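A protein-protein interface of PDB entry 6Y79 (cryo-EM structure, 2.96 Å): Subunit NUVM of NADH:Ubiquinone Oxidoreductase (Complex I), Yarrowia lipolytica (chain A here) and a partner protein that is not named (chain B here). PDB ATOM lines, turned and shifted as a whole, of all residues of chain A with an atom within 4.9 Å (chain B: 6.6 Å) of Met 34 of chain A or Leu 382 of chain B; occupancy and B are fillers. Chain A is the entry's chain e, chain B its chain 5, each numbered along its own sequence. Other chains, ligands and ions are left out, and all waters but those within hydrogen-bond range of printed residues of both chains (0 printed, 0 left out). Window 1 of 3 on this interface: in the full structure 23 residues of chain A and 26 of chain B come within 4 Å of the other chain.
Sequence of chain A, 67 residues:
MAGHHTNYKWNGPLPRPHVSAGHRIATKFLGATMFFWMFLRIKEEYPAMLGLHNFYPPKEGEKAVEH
Among the printed residues, merely in contact across the chains: Gly 31 of chain A with Ile 375 of chain B (3.9 Å), Thr 33 of chain A with Met 470 of chain B (3.7 Å), Met 34 of chain A with Ile 375 of chain B (3.8 Å), Met 34 of chain A with Ile 379 of chain B (3.6 Å), Met 34 of chain A with Leu 382 of chain B (3.7 Å), Met 34 of chain A with Met 470 of chain B (3.7 Å), Met 38 of chain A with Pro 388 of chain B (3.3 Å) and Met 38 of chain A with Leu 390 of chain B (3.8 Å).
Printed residues of chain B within 4 Å of Gly 31 of chain A: Ile 375. Printed residues of chain B within 4 Å of Thr 33 of chain A: Met 470. Met 34 of chain A touches just these residues of chain B: Ile 375 (3.8 Å), Ile 379 (3.6 Å), Leu 382 (3.7 Å) and Met 470 (3.7 Å). Of the printed residues of chain A, Ile 375 of chain B touches Gly 31 and Met 34. Of chain A, only Met 34 (3.7 Å) comes within 4 Å of Leu 382 of chain B. Printed residues of chain A within 4 Å of Leu 390 of chain B: Met 38 (3.8 Å). The nearest residue of chain B that does not touch Met 34 of chain A is Leu 390 of chain B (4.6 Å). The nearest printed residue of chain A that does not touch Leu 382 of chain B is Met 38 of chain A (4.9 Å). The nearest printed residue of chain B that does not touch Gly 31 of chain A is Ile 379 of chain B (5.5 Å).
The backbone carbonyl oxygen (O) of Ile 379 of chain B sits at hydrogen-bond distance from the side-chain hydroxyl (OG) of Ser 383 of chain B (3.1 Å). O of Leu 382 of chain B sits at hydrogen-bond distance from N of Met 387 of chain B, at 3.2 Å.
Printed residues of chain A that touch a printed residue of chain B: Gly 31, Thr 33, Met 34 and Met 38. Hydrophobic or aromatic side chains of chain A within 4 Å of the printed part of chain B: Met 34 and Met 38.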
ATOM      1  N   LEU A  30      12.209 -10.361 -12.107  1.00  0.00           N
ATOM      2  CA  LEU A  30      11.797 -10.687 -13.475  1.00  0.00           C
ATOM      3  C   LEU A  30      10.298 -10.483 -13.684  1.00  0.00           C
ATOM      4  O   LEU A  30       9.875  -9.947 -14.719  1.00  0.00           O
ATOM      5  CB  LEU A  30      12.189 -12.124 -13.821  1.00  0.00           C
ATOM      6  CG  LEU A  30      13.655 -12.357 -14.182  1.00  0.00           C
ATOM      7  CD1 LEU A  30      13.911 -13.820 -14.493  1.00  0.00           C
ATOM      8  CD2 LEU A  30      14.048 -11.489 -15.356  1.00  0.00           C
ATOM      9  N   GLY A  31       9.483 -10.876 -12.703  1.00  0.00           N
ATOM     10  CA  GLY A  31       8.048 -10.673 -12.816  1.00  0.00           C
ATOM     11  C   GLY A  31       7.645  -9.212 -12.739  1.00  0.00           C
ATOM     12  O   GLY A  31       6.741  -8.767 -13.454  1.00  0.00           O
ATOM     13  N   ALA A  32       8.304  -8.440 -11.873  1.00  0.00           N
ATOM     14  CA  ALA A  32       8.020  -7.014 -11.806  1.00  0.00           C
ATOM     15  C   ALA A  32       8.411  -6.320 -13.102  1.00  0.00           C
ATOM     16  O   ALA A  32       7.669  -5.462 -13.598  1.00  0.00           O
ATOM     17  CB  ALA A  32       8.744  -6.397 -10.613  1.00  0.00           C
ATOM     18  N   THR A  33       9.545  -6.730 -13.693  1.00  0.00           N
ATOM     19  CA  THR A  33       9.995  -6.172 -14.962  1.00  0.00           C
ATOM     20  C   THR A  33       9.011  -6.468 -16.090  1.00  0.00           C
ATOM     21  O   THR A  33       8.667  -5.559 -16.854  1.00  0.00           O
ATOM     22  CB  THR A  33      11.379  -6.723 -15.301  1.00  0.00           C
ATOM     23  OG1 THR A  33      12.302  -6.367 -14.272  1.00  0.00           O
ATOM     24  CG2 THR A  33      11.882  -6.161 -16.609  1.00  0.00           C
ATOM     25  N   MET A  34       8.485  -7.701 -16.154  1.00  0.00           N
ATOM     26  CA  MET A  34       7.568  -8.081 -17.230  1.00  0.00           C
ATOM     27  C   MET A  34       6.213  -7.380 -17.101  1.00  0.00           C
ATOM     28  O   MET A  34       5.685  -6.871 -18.096  1.00  0.00           O
ATOM     29  CB  MET A  34       7.399  -9.610 -17.291  1.00  0.00           C
ATOM     30  CG  MET A  34       6.645 -10.315 -16.174  1.00  0.00           C
ATOM     31  SD  MET A  34       6.326 -12.040 -16.457  1.00  0.00           S
ATOM     32  CE  MET A  34       5.577 -11.812 -18.073  1.00  0.00           C
ATOM     33  N   PHE A  35       5.644  -7.312 -15.876  1.00  0.00           N
ATOM     34  CA  PHE A  35       4.326  -6.702 -15.749  1.00  0.00           C
ATOM     35  C   PHE A  35       4.420  -5.186 -15.891  1.00  0.00           C
ATOM     36  O   PHE A  35       3.530  -4.561 -16.485  1.00  0.00           O
ATOM     37  CB  PHE A  35       3.687  -7.077 -14.425  1.00  0.00           C
ATOM     38  CG  PHE A  35       3.114  -8.479 -14.366  1.00  0.00           C
ATOM     39  CD1 PHE A  35       1.992  -8.824 -15.093  1.00  0.00           C
ATOM     40  CD2 PHE A  35       3.684  -9.437 -13.539  1.00  0.00           C
ATOM     41  CE1 PHE A  35       1.464 -10.110 -15.030  1.00  0.00           C
ATOM     42  CE2 PHE A  35       3.170 -10.719 -13.470  1.00  0.00           C
ATOM     43  CZ  PHE A  35       2.058 -11.058 -14.214  1.00  0.00           C
ATOM     44  N   PHE A  36       5.536  -4.594 -15.443  1.00  0.00           N
ATOM     45  CA  PHE A  36       5.736  -3.161 -15.603  1.00  0.00           C
ATOM     46  C   PHE A  36       5.954  -2.792 -17.064  1.00  0.00           C
ATOM     47  O   PHE A  36       5.385  -1.808 -17.555  1.00  0.00           O
ATOM     48  CB  PHE A  36       6.918  -2.722 -14.751  1.00  0.00           C
ATOM     49  CG  PHE A  36       7.211  -1.266 -14.837  1.00  0.00           C
ATOM     50  CD1 PHE A  36       6.392  -0.350 -14.208  1.00  0.00           C
ATOM     51  CD2 PHE A  36       8.302  -0.807 -15.550  1.00  0.00           C
ATOM     52  CE1 PHE A  36       6.657   0.999 -14.289  1.00  0.00           C
ATOM     53  CE2 PHE A  36       8.570   0.539 -15.635  1.00  0.00           C
ATOM     54  CZ  PHE A  36       7.746   1.444 -15.004  1.00  0.00           C
ATOM     55  N   TRP A  37       6.779  -3.569 -17.774  1.00  0.00           N
ATOM     56  CA  TRP A  37       7.041  -3.288 -19.177  1.00  0.00           C
ATOM     57  C   TRP A  37       5.804  -3.504 -20.030  1.00  0.00           C
ATOM     58  O   TRP A  37       5.547  -2.720 -20.953  1.00  0.00           O
ATOM     59  CB  TRP A  37       8.180  -4.165 -19.681  1.00  0.00           C
ATOM     60  CG  TRP A  37       8.544  -3.874 -21.088  1.00  0.00           C
ATOM     61  CD1 TRP A  37       8.289  -4.647 -22.176  1.00  0.00           C
ATOM     62  CD2 TRP A  37       9.213  -2.709 -21.568  1.00  0.00           C
ATOM     63  NE1 TRP A  37       8.770  -4.041 -23.308  1.00  0.00           N
ATOM     64  CE2 TRP A  37       9.341  -2.848 -22.959  1.00  0.00           C
ATOM     65  CE3 TRP A  37       9.724  -1.564 -20.954  1.00  0.00           C
ATOM     66  CZ2 TRP A  37       9.958  -1.885 -23.746  1.00  0.00           C
ATOM     67  CZ3 TRP A  37      10.337  -0.611 -21.737  1.00  0.00           C
ATOM     68  CH2 TRP A  37      10.448  -0.776 -23.117  1.00  0.00           C
ATOM     69  N   MET A  38       5.011  -4.533 -19.718  1.00  0.00           N
ATOM     70  CA  MET A  38       3.779  -4.748 -20.459  1.00  0.00           C
ATOM     71  C   MET A  38       2.769  -3.647 -20.181  1.00  0.00           C
ATOM     72  O   MET A  38       2.081  -3.212 -21.102  1.00  0.00           O
ATOM     73  CB  MET A  38       3.197  -6.125 -20.144  1.00  0.00           C
ATOM     74  CG  MET A  38       3.979  -7.260 -20.783  1.00  0.00           C
ATOM     75  SD  MET A  38       3.431  -8.882 -20.240  1.00  0.00           S
ATOM     76  CE  MET A  38       1.982  -9.087 -21.259  1.00  0.00           C
ATOM     77  N   PHE A  39       2.706  -3.141 -18.945  1.00  0.00           N
ATOM     78  CA  PHE A  39       1.799  -2.032 -18.662  1.00  0.00           C
ATOM     79  C   PHE A  39       2.222  -0.760 -19.382  1.00  0.00           C
ATOM     80  O   PHE A  39       1.371  -0.041 -19.914  1.00  0.00           O
ATOM     81  CB  PHE A  39       1.714  -1.778 -17.161  1.00  0.00           C
ATOM     82  CG  PHE A  39       0.924  -2.806 -16.417  1.00  0.00           C
ATOM     83  CD1 PHE A  39       0.075  -3.676 -17.085  1.00  0.00           C
ATOM     84  CD2 PHE A  39       1.033  -2.906 -15.043  1.00  0.00           C
ATOM     85  CE1 PHE A  39      -0.644  -4.623 -16.396  1.00  0.00           C
ATOM     86  CE2 PHE A  39       0.315  -3.852 -14.348  1.00  0.00           C
ATOM     87  CZ  PHE A  39      -0.525  -4.710 -15.027  1.00  0.00           C
ATOM     88  N   ILE B 375       8.894 -18.450 -13.592  1.00  0.00           N
ATOM     89  CA  ILE B 375       8.780 -17.088 -14.101  1.00  0.00           C
ATOM     90  C   ILE B 375       9.423 -16.983 -15.478  1.00  0.00           C
ATOM     91  O   ILE B 375       8.894 -16.287 -16.354  1.00  0.00           O
ATOM     92  CB  ILE B 375       9.334 -16.051 -13.095  1.00  0.00           C
ATOM     93  CG1 ILE B 375       8.948 -14.633 -13.514  1.00  0.00           C
ATOM     94  CG2 ILE B 375      10.844 -16.115 -12.941  1.00  0.00           C
ATOM     95  CD1 ILE B 375       7.483 -14.439 -13.798  1.00  0.00           C
ATOM     96  N   ILE B 377       9.615 -19.530 -17.782  1.00  0.00           N
ATOM     97  CA  ILE B 377       8.743 -20.212 -18.734  1.00  0.00           C
ATOM     98  C   ILE B 377       7.440 -19.444 -18.945  1.00  0.00           C
ATOM     99  O   ILE B 377       6.867 -19.482 -20.040  1.00  0.00           O
ATOM    100  CB  ILE B 377       8.521 -21.677 -18.276  1.00  0.00           C
ATOM    101  CG1 ILE B 377       7.983 -22.531 -19.409  1.00  0.00           C
ATOM    102  CG2 ILE B 377       7.555 -21.797 -17.145  1.00  0.00           C
ATOM    103  CD1 ILE B 377       7.975 -24.002 -19.102  1.00  0.00           C
ATOM    104  N   THR B 378       7.012 -18.657 -17.954  1.00  0.00           N
ATOM    105  CA  THR B 378       5.857 -17.789 -18.109  1.00  0.00           C
ATOM    106  C   THR B 378       6.155 -16.607 -19.013  1.00  0.00           C
ATOM    107  O   THR B 378       5.300 -16.251 -19.833  1.00  0.00           O
ATOM    108  CB  THR B 378       5.391 -17.309 -16.733  1.00  0.00           C
ATOM    109  OG1 THR B 378       5.272 -18.436 -15.859  1.00  0.00           O
ATOM    110  CG2 THR B 378       4.046 -16.610 -16.815  1.00  0.00           C
ATOM    111  N   ILE B 379       7.351 -16.014 -18.887  1.00  0.00           N
ATOM    112  CA  ILE B 379       7.776 -14.974 -19.825  1.00  0.00           C
ATOM    113  C   ILE B 379       7.831 -15.529 -21.253  1.00  0.00           C
ATOM    114  O   ILE B 379       7.304 -14.917 -22.197  1.00  0.00           O
ATOM    115  CB  ILE B 379       9.143 -14.393 -19.414  1.00  0.00           C
ATOM    116  CG1 ILE B 379       9.072 -13.610 -18.137  1.00  0.00           C
ATOM    117  CG2 ILE B 379       9.657 -13.458 -20.486  1.00  0.00           C
ATOM    118  CD1 ILE B 379      10.423 -13.267 -17.580  1.00  0.00           C
ATOM    119  N   ALA B 380       8.398 -16.734 -21.411  1.00  0.00           N
ATOM    120  CA  ALA B 380       8.578 -17.329 -22.733  1.00  0.00           C
ATOM    121  C   ALA B 380       7.246 -17.640 -23.391  1.00  0.00           C
ATOM    122  O   ALA B 380       7.071 -17.400 -24.589  1.00  0.00           O
ATOM    123  CB  ALA B 380       9.421 -18.594 -22.615  1.00  0.00           C
ATOM    124  N   SER B 381       6.281 -18.143 -22.617  1.00  0.00           N
ATOM    125  CA  SER B 381       5.008 -18.527 -23.212  1.00  0.00           C
ATOM    126  C   SER B 381       4.072 -17.337 -23.386  1.00  0.00           C
ATOM    127  O   SER B 381       3.256 -17.329 -24.313  1.00  0.00           O
ATOM    128  CB  SER B 381       4.359 -19.619 -22.379  1.00  0.00           C
ATOM    129  OG  SER B 381       5.116 -20.807 -22.489  1.00  0.00           O
ATOM    130  N   LEU B 382       4.172 -16.316 -22.526  1.00  0.00           N
ATOM    131  CA  LEU B 382       3.399 -15.105 -22.772  1.00  0.00           C
ATOM    132  C   LEU B 382       3.939 -14.350 -23.977  1.00  0.00           C
ATOM    133  O   LEU B 382       3.185 -13.647 -24.656  1.00  0.00           O
ATOM    134  CB  LEU B 382       3.388 -14.206 -21.536  1.00  0.00           C
ATOM    135  CG  LEU B 382       2.439 -14.594 -20.399  1.00  0.00           C
ATOM    136  CD1 LEU B 382       2.591 -13.647 -19.229  1.00  0.00           C
ATOM    137  CD2 LEU B 382       1.028 -14.583 -20.848  1.00  0.00           C
ATOM    138  N   SER B 383       5.235 -14.492 -24.260  1.00  0.00           N
ATOM    139  CA  SER B 383       5.789 -13.933 -25.483  1.00  0.00           C
ATOM    140  C   SER B 383       5.398 -14.747 -26.712  1.00  0.00           C
ATOM    141  O   SER B 383       5.078 -14.162 -27.746  1.00  0.00           O
ATOM    142  CB  SER B 383       7.308 -13.844 -25.372  1.00  0.00           C
ATOM    143  OG  SER B 383       7.700 -12.856 -24.450  1.00  0.00           O
ATOM    144  N   LEU B 384       5.386 -16.085 -26.628  1.00  0.00           N
ATOM    145  CA  LEU B 384       5.054 -16.869 -27.819  1.00  0.00           C
ATOM    146  C   LEU B 384       3.568 -16.840 -28.130  1.00  0.00           C
ATOM    147  O   LEU B 384       3.175 -17.039 -29.286  1.00  0.00           O
ATOM    148  CB  LEU B 384       5.552 -18.307 -27.654  1.00  0.00           C
ATOM    149  CG  LEU B 384       5.671 -19.081 -28.974  1.00  0.00           C
ATOM    150  CD1 LEU B 384       6.995 -19.785 -29.054  1.00  0.00           C
ATOM    151  CD2 LEU B 384       4.557 -20.099 -29.182  1.00  0.00           C
ATOM    152  N   MET B 385       2.740 -16.525 -27.142  1.00  0.00           N
ATOM    153  CA  MET B 385       1.325 -16.310 -27.372  1.00  0.00           C
ATOM    154  C   MET B 385       1.022 -14.907 -27.875  1.00  0.00           C
ATOM    155  O   MET B 385      -0.159 -14.568 -28.032  1.00  0.00           O
ATOM    156  CB  MET B 385       0.537 -16.581 -26.098  1.00  0.00           C
ATOM    157  CG  MET B 385       0.404 -18.055 -25.769  1.00  0.00           C
ATOM    158  SD  MET B 385      -0.597 -18.337 -24.321  1.00  0.00           S
ATOM    159  CE  MET B 385       0.131 -17.109 -23.273  1.00  0.00           C
ATOM    160  N   ALA B 386       2.064 -14.102 -28.122  1.00  0.00           N
ATOM    161  CA  ALA B 386       1.976 -12.755 -28.691  1.00  0.00           C
ATOM    162  C   ALA B 386       1.127 -11.828 -27.828  1.00  0.00           C
ATOM    163  O   ALA B 386       0.336 -11.032 -28.335  1.00  0.00           O
ATOM    164  CB  ALA B 386       1.477 -12.786 -30.140  1.00  0.00           C
ATOM    165  N   MET B 387       1.274 -11.954 -26.512  1.00  0.00           N
ATOM    166  CA  MET B 387       0.568 -11.062 -25.612  1.00  0.00           C
ATOM    167  C   MET B 387       1.358  -9.775 -25.416  1.00  0.00           C
ATOM    168  O   MET B 387       2.577  -9.817 -25.212  1.00  0.00           O
ATOM    169  CB  MET B 387       0.284 -11.740 -24.277  1.00  0.00           C
ATOM    170  CG  MET B 387      -0.870 -12.680 -24.414  1.00  0.00           C
ATOM    171  SD  MET B 387      -1.520 -13.160 -22.830  1.00  0.00           S
ATOM    172  CE  MET B 387      -2.498 -14.554 -23.353  1.00  0.00           C
ATOM    173  N   PRO B 388       0.688  -8.629 -25.430  1.00  0.00           N
ATOM    174  CA  PRO B 388       1.331  -7.415 -25.940  1.00  0.00           C
ATOM    175  C   PRO B 388       2.291  -6.747 -24.974  1.00  0.00           C
ATOM    176  O   PRO B 388       2.189  -6.870 -23.753  1.00  0.00           O
ATOM    177  CB  PRO B 388       0.150  -6.500 -26.265  1.00  0.00           C
ATOM    178  CG  PRO B 388      -0.963  -7.020 -25.481  1.00  0.00           C
ATOM    179  CD  PRO B 388      -0.764  -8.462 -25.250  1.00  0.00           C
ATOM    180  N   LEU B 390       5.437  -7.609 -25.300  1.00  0.00           N
ATOM    181  CA  LEU B 390       6.538  -8.545 -25.424  1.00  0.00           C
ATOM    182  C   LEU B 390       6.861  -8.767 -26.893  1.00  0.00           C
ATOM    183  O   LEU B 390       6.128  -8.330 -27.782  1.00  0.00           O
ATOM    184  CB  LEU B 390       6.205  -9.869 -24.729  1.00  0.00           C
ATOM    185  CG  LEU B 390       5.976  -9.733 -23.217  1.00  0.00           C
ATOM    186  CD1 LEU B 390       5.556 -11.044 -22.593  1.00  0.00           C
ATOM    187  CD2 LEU B 390       7.211  -9.200 -22.530  1.00  0.00           C
ATOM    188  N   GLY B 392       6.820 -11.294 -28.942  1.00  0.00           N
ATOM    189  CA  GLY B 392       5.989 -12.054 -29.850  1.00  0.00           C
ATOM    190  C   GLY B 392       4.797 -11.310 -30.384  1.00  0.00           C
ATOM    191  O   GLY B 392       4.285 -11.684 -31.439  1.00  0.00           O
ATOM    192  N   TYR B 393       4.320 -10.292 -29.654  1.00  0.00           N
ATOM    193  CA  TYR B 393       3.367  -9.338 -30.210  1.00  0.00           C
ATOM    194  C   TYR B 393       3.863  -8.825 -31.555  1.00  0.00           C
ATOM    195  O   TYR B 393       3.281  -9.121 -32.608  1.00  0.00           O
ATOM    196  CB  TYR B 393       3.143  -8.159 -29.248  1.00  0.00           C
ATOM    197  CG  TYR B 393       2.095  -7.210 -29.788  1.00  0.00           C
ATOM    198  CD1 TYR B 393       0.753  -7.493 -29.629  1.00  0.00           C
ATOM    199  CD2 TYR B 393       2.443  -6.079 -30.520  1.00  0.00           C
ATOM    200  CE1 TYR B 393      -0.211  -6.673 -30.147  1.00  0.00           C
ATOM    201  CE2 TYR B 393       1.484  -5.262 -31.063  1.00  0.00           C
ATOM    202  CZ  TYR B 393       0.160  -5.566 -30.868  1.00  0.00           C
ATOM    203  OH  TYR B 393      -0.814  -4.751 -31.389  1.00  0.00           O
ATOM    204  N   SER B 429       0.164 -24.415 -24.795  1.00  0.00           N
ATOM    205  CA  SER B 429       1.076 -23.659 -23.953  1.00  0.00           C
ATOM    206  C   SER B 429       0.545 -23.588 -22.538  1.00  0.00           C
ATOM    207  O   SER B 429       1.299 -23.818 -21.579  1.00  0.00           O
ATOM    208  CB  SER B 429       1.278 -22.260 -24.529  1.00  0.00           C
ATOM    209  OG  SER B 429       1.796 -21.391 -23.548  1.00  0.00           O
ATOM    210  N   MET B 430      -0.774 -23.409 -22.405  1.00  0.00           N
ATOM    211  CA  MET B 430      -1.354 -23.402 -21.076  1.00  0.00           C
ATOM    212  C   MET B 430      -1.308 -24.782 -20.453  1.00  0.00           C
ATOM    213  O   MET B 430      -1.100 -24.890 -19.240  1.00  0.00           O
ATOM    214  CB  MET B 430      -2.772 -22.884 -21.145  1.00  0.00           C
ATOM    215  CG  MET B 430      -2.874 -21.431 -21.537  1.00  0.00           C
ATOM    216  SD  MET B 430      -2.300 -20.338 -20.229  1.00  0.00           S
ATOM    217  CE  MET B 430      -0.777 -19.743 -20.920  1.00  0.00           C
ATOM    218  N   MET B 470      12.134 -10.301 -23.787  1.00  0.00           N
ATOM    219  CA  MET B 470      11.221  -9.209 -23.492  1.00  0.00           C
ATOM    220  C   MET B 470      11.491  -7.953 -24.322  1.00  0.00           C
ATOM    221  O   MET B 470      10.548  -7.343 -24.833  1.00  0.00           O
ATOM    222  CB  MET B 470      11.289  -8.879 -22.012  1.00  0.00           C
ATOM    223  CG  MET B 470      10.614  -9.897 -21.128  1.00  0.00           C
ATOM    224  SD  MET B 470      10.752  -9.373 -19.421  1.00  0.00           S
ATOM    225  CE  MET B 470      10.334  -7.647 -19.627  1.00  0.00           C
ATOM    226  N   ILE B 519      -6.064 -14.095 -25.327  1.00  0.00           N
ATOM    227  CA  ILE B 519      -6.050 -14.047 -23.864  1.00  0.00           C
ATOM    228  C   ILE B 519      -7.273 -14.763 -23.276  1.00  0.00           C
ATOM    229  O   ILE B 519      -7.180 -15.420 -22.225  1.00  0.00           O
ATOM    230  CB  ILE B 519      -5.877 -12.603 -23.348  1.00  0.00           C
ATOM    231  CG1 ILE B 519      -5.400 -12.630 -21.898  1.00  0.00           C
ATOM    232  CG2 ILE B 519      -7.118 -11.749 -23.472  1.00  0.00           C
ATOM    233  CD1 ILE B 519      -4.647 -11.404 -21.476  1.00  0.00           C
ATOM    234  N   SER B 522      -6.785 -18.624 -23.363  1.00  0.00           N
ATOM    235  CA  SER B 522      -5.802 -19.015 -22.350  1.00  0.00           C
ATOM    236  C   SER B 522      -6.413 -19.058 -20.952  1.00  0.00           C
ATOM    237  O   SER B 522      -6.236 -20.038 -20.203  1.00  0.00           O
ATOM    238  CB  SER B 522      -4.622 -18.051 -22.376  1.00  0.00           C
ATOM    239  OG  SER B 522      -5.040 -16.780 -21.925  1.00  0.00           O
